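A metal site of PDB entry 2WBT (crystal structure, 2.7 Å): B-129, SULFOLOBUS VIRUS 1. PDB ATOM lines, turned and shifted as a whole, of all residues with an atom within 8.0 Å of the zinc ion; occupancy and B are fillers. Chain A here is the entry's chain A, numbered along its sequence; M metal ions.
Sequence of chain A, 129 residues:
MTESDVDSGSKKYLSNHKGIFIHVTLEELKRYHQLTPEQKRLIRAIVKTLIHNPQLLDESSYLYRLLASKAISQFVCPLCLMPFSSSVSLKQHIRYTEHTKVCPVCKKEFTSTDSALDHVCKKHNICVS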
ATOM      1  N   GLU A  59      -9.557  10.470   6.277  1.00  0.00           N
ATOM      2  CA  GLU A  59     -10.353   9.799   7.319  1.00  0.00           C
ATOM      3  C   GLU A  59      -9.931   8.337   7.528  1.00  0.00           C
ATOM      4  O   GLU A  59     -10.529   7.636   8.346  1.00  0.00           O
ATOM      5  CB  GLU A  59     -11.837   9.841   6.929  1.00  0.00           C
ATOM      6  CG  GLU A  59     -12.450  11.232   6.868  1.00  0.00           C
ATOM      7  CD  GLU A  59     -13.820  11.255   6.216  1.00  0.00           C
ATOM      8  OE1 GLU A  59     -14.455  10.179   6.111  1.00  0.00           O
ATOM      9  OE2 GLU A  59     -14.274  12.344   5.804  1.00  0.00           O
ATOM     10  N   VAL A 102     -13.478  17.897  19.455  1.00  0.00           N
ATOM     11  CA  VAL A 102     -13.228  17.770  18.017  1.00  0.00           C
ATOM     12  C   VAL A 102     -13.637  16.383  17.536  1.00  0.00           C
ATOM     13  O   VAL A 102     -13.377  15.384  18.201  1.00  0.00           O
ATOM     14  CB  VAL A 102     -11.736  17.993  17.668  1.00  0.00           C
ATOM     15  CG1 VAL A 102     -11.566  18.166  16.170  1.00  0.00           C
ATOM     16  CG2 VAL A 102     -11.190  19.201  18.413  1.00  0.00           C
ATOM     17  N   CYS A 103     -14.277  16.349  16.374  1.00  0.00           N
ATOM     18  CA  CYS A 103     -14.660  15.081  15.743  1.00  0.00           C
ATOM     19  C   CYS A 103     -13.429  14.423  15.118  1.00  0.00           C
ATOM     20  O   CYS A 103     -12.786  15.045  14.257  1.00  0.00           O
ATOM     21  CB  CYS A 103     -15.743  15.307  14.696  1.00  0.00           C
ATOM     22  SG  CYS A 103     -16.093  13.856  13.660  1.00  0.00           S
ATOM     23  N   PRO A 104     -13.108  13.167  15.531  1.00  0.00           N
ATOM     24  CA  PRO A 104     -11.884  12.497  15.081  1.00  0.00           C
ATOM     25  C   PRO A 104     -11.842  12.294  13.564  1.00  0.00           C
ATOM     26  O   PRO A 104     -10.777  12.005  13.009  1.00  0.00           O
ATOM     27  CB  PRO A 104     -11.948  11.143  15.789  1.00  0.00           C
ATOM     28  CG  PRO A 104     -13.372  10.923  16.075  1.00  0.00           C
ATOM     29  CD  PRO A 104     -13.895  12.288  16.413  1.00  0.00           C
ATOM     30  N   VAL A 105     -12.988  12.441  12.911  1.00  0.00           N
ATOM     31  CA  VAL A 105     -13.145  12.199  11.486  1.00  0.00           C
ATOM     32  C   VAL A 105     -12.980  13.469  10.655  1.00  0.00           C
ATOM     33  O   VAL A 105     -12.077  13.558   9.811  1.00  0.00           O
ATOM     34  CB  VAL A 105     -14.528  11.571  11.174  1.00  0.00           C
ATOM     35  CG1 VAL A 105     -14.602  11.122   9.736  1.00  0.00           C
ATOM     36  CG2 VAL A 105     -14.807  10.400  12.121  1.00  0.00           C
ATOM     37  N   CYS A 106     -13.836  14.460  10.898  1.00  0.00           N
ATOM     38  CA  CYS A 106     -13.888  15.691  10.077  1.00  0.00           C
ATOM     39  C   CYS A 106     -13.210  16.912  10.691  1.00  0.00           C
ATOM     40  O   CYS A 106     -12.994  17.898   9.998  1.00  0.00           O
ATOM     41  CB  CYS A 106     -15.338  16.027   9.729  1.00  0.00           C
ATOM     42  SG  CYS A 106     -16.242  16.852  11.049  1.00  0.00           S
ATOM     43  N   LYS A 107     -12.908  16.858  11.980  1.00  0.00           N
ATOM     44  CA  LYS A 107     -12.158  17.929  12.662  1.00  0.00           C
ATOM     45  C   LYS A 107     -12.961  19.190  12.945  1.00  0.00           C
ATOM     46  O   LYS A 107     -12.390  20.273  13.134  1.00  0.00           O
ATOM     47  CB  LYS A 107     -10.888  18.272  11.878  1.00  0.00           C
ATOM     48  CG  LYS A 107      -9.954  17.103  11.701  1.00  0.00           C
ATOM     49  CD  LYS A 107      -9.225  16.808  12.995  1.00  0.00           C
ATOM     50  CE  LYS A 107      -8.768  15.366  13.069  1.00  0.00           C
ATOM     51  NZ  LYS A 107      -7.615  15.201  13.990  1.00  0.00           N
ATOM     52  N   LYS A 108     -14.281  19.039  12.989  1.00  0.00           N
ATOM     53  CA  LYS A 108     -15.194  20.120  13.309  1.00  0.00           C
ATOM     54  C   LYS A 108     -15.305  20.236  14.833  1.00  0.00           C
ATOM     55  O   LYS A 108     -15.269  19.215  15.529  1.00  0.00           O
ATOM     56  CB  LYS A 108     -16.557  19.832  12.699  1.00  0.00           C
ATOM     57  CG  LYS A 108     -17.546  20.951  12.822  1.00  0.00           C
ATOM     58  CD  LYS A 108     -18.916  20.488  12.385  1.00  0.00           C
ATOM     59  CE  LYS A 108     -19.961  21.333  13.031  1.00  0.00           C
ATOM     60  NZ  LYS A 108     -21.322  20.996  12.507  1.00  0.00           N
ATOM     61  N   GLU A 109     -15.459  21.458  15.339  1.00  0.00           N
ATOM     62  CA  GLU A 109     -15.426  21.698  16.796  1.00  0.00           C
ATOM     63  C   GLU A 109     -16.791  22.044  17.395  1.00  0.00           C
ATOM     64  O   GLU A 109     -17.687  22.501  16.691  1.00  0.00           O
ATOM     65  CB  GLU A 109     -14.389  22.777  17.125  1.00  0.00           C
ATOM     66  CG  GLU A 109     -13.625  22.507  18.412  1.00  0.00           C
ATOM     67  CD  GLU A 109     -12.626  23.585  18.775  1.00  0.00           C
ATOM     68  OE1 GLU A 109     -12.309  24.432  17.901  1.00  0.00           O
ATOM     69  OE2 GLU A 109     -12.155  23.597  19.923  1.00  0.00           O
ATOM     70  N   PHE A 110     -16.927  21.807  18.702  1.00  0.00           N
ATOM     71  CA  PHE A 110     -18.219  21.921  19.390  1.00  0.00           C
ATOM     72  C   PHE A 110     -18.133  22.509  20.798  1.00  0.00           C
ATOM     73  O   PHE A 110     -17.057  22.624  21.377  1.00  0.00           O
ATOM     74  CB  PHE A 110     -18.899  20.551  19.463  1.00  0.00           C
ATOM     75  CG  PHE A 110     -19.085  19.913  18.115  1.00  0.00           C
ATOM     76  CD1 PHE A 110     -18.102  19.071  17.594  1.00  0.00           C
ATOM     77  CD2 PHE A 110     -20.225  20.157  17.361  1.00  0.00           C
ATOM     78  CE1 PHE A 110     -18.258  18.490  16.352  1.00  0.00           C
ATOM     79  CE2 PHE A 110     -20.390  19.577  16.124  1.00  0.00           C
ATOM     80  CZ  PHE A 110     -19.402  18.742  15.609  1.00  0.00           C
ATOM     81  N   ALA A 116     -20.355  16.777  20.037  1.00  0.00           N
ATOM     82  CA  ALA A 116     -19.375  16.030  19.234  1.00  0.00           C
ATOM     83  C   ALA A 116     -19.852  14.598  18.970  1.00  0.00           C
ATOM     84  O   ALA A 116     -19.637  14.064  17.878  1.00  0.00           O
ATOM     85  CB  ALA A 116     -18.026  16.019  19.925  1.00  0.00           C
ATOM     86  N   HIS A 119     -22.837  14.566  16.472  1.00  0.00           N
ATOM     87  CA  HIS A 119     -22.271  14.851  15.148  1.00  0.00           C
ATOM     88  C   HIS A 119     -21.659  13.615  14.499  1.00  0.00           C
ATOM     89  O   HIS A 119     -21.930  13.328  13.330  1.00  0.00           O
ATOM     90  CB  HIS A 119     -21.234  15.985  15.228  1.00  0.00           C
ATOM     91  CG  HIS A 119     -20.314  16.042  14.051  1.00  0.00           C
ATOM     92  ND1 HIS A 119     -20.625  16.698  12.872  1.00  0.00           N
ATOM     93  CD2 HIS A 119     -19.070  15.540  13.887  1.00  0.00           C
ATOM     94  CE1 HIS A 119     -19.623  16.579  12.022  1.00  0.00           C
ATOM     95  NE2 HIS A 119     -18.653  15.878  12.618  1.00  0.00           N
ATOM     96  N   VAL A 120     -20.832  12.890  15.251  1.00  0.00           N
ATOM     97  CA  VAL A 120     -20.171  11.689  14.721  1.00  0.00           C
ATOM     98  C   VAL A 120     -21.177  10.592  14.371  1.00  0.00           C
ATOM     99  O   VAL A 120     -20.902   9.728  13.533  1.00  0.00           O
ATOM    100  CB  VAL A 120     -19.094  11.158  15.699  1.00  0.00           C
ATOM    101  CG1 VAL A 120     -18.460   9.880  15.164  1.00  0.00           C
ATOM    102  CG2 VAL A 120     -18.032  12.212  15.944  1.00  0.00           C
ATOM    103  N   CYS A 121     -22.343  10.619  15.012  1.00  0.00           N
ATOM    104  CA  CYS A 121     -23.422   9.695  14.696  1.00  0.00           C
ATOM    105  C   CYS A 121     -24.274  10.189  13.519  1.00  0.00           C
ATOM    106  O   CYS A 121     -24.613   9.413  12.627  1.00  0.00           O
ATOM    107  CB  CYS A 121     -24.322   9.484  15.917  1.00  0.00           C
ATOM    108  SG  CYS A 121     -25.725   8.368  15.629  1.00  0.00           S
ATOM    109  N   LYS A 123     -23.607  12.644  11.108  1.00  0.00           N
ATOM    110  CA  LYS A 123     -22.925  12.918   9.834  1.00  0.00           C
ATOM    111  C   LYS A 123     -21.776  11.966   9.496  1.00  0.00           C
ATOM    112  O   LYS A 123     -21.169  12.094   8.432  1.00  0.00           O
ATOM    113  CB  LYS A 123     -22.468  14.380   9.787  1.00  0.00           C
ATOM    114  CG  LYS A 123     -23.558  15.304   9.270  1.00  0.00           C
ATOM    115  CD  LYS A 123     -23.345  16.755   9.659  1.00  0.00           C
ATOM    116  CE  LYS A 123     -22.255  17.408   8.829  1.00  0.00           C
ATOM    117  NZ  LYS A 123     -22.124  18.849   9.188  1.00  0.00           N
ATOM    118  N   HIS A 124     -21.454  11.025  10.389  1.00  0.00           N
ATOM    119  CA  HIS A 124     -20.485   9.976  10.073  1.00  0.00           C
ATOM    120  C   HIS A 124     -21.019   8.569  10.339  1.00  0.00           C
ATOM    121  O   HIS A 124     -20.373   7.571   9.982  1.00  0.00           O
ATOM    122  CB  HIS A 124     -19.180  10.210  10.827  1.00  0.00           C
ATOM    123  CG  HIS A 124     -18.586  11.555  10.574  1.00  0.00           C
ATOM    124  ND1 HIS A 124     -17.863  11.831   9.434  1.00  0.00           N
ATOM    125  CD2 HIS A 124     -18.637  12.715  11.268  1.00  0.00           C
ATOM    126  CE1 HIS A 124     -17.477  13.098   9.450  1.00  0.00           C
ATOM    127  NE2 HIS A 124     -17.933  13.645  10.558  1.00  0.00           N
HETATM  128 ZN    ZN M   1     -16.938  15.038  11.924  1.00  0.00          ZN
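The side-chain sulfur (SG) of Cys 106 lies close to the backbone NH (N) of Lys 108 (3.5 Å). N of Val 105 sits close to SG of Cys 103. The backbone NH (N) of Cys 103 is in hydrogen-bond range of the backbone carbonyl oxygen (O) of Lys 108 (3.1 Å).
Of the 16 residues printed, 4 come within 4 Å of the zinc ion. The nearest printed residue that does not touch the zinc ion is Val 105 (4.3 Å).
NE2 of His 119 binds the zinc ion. The side-chain sulfur (SG) of Cys 106 binds the zinc ion (2.1 Å). The zinc ion is bound by NE2 of His 124, at 2.2 Å. SG of Cys 103 binds the zinc ion, at 2.3 Å. The zinc ion has four donor atoms within binding distance.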
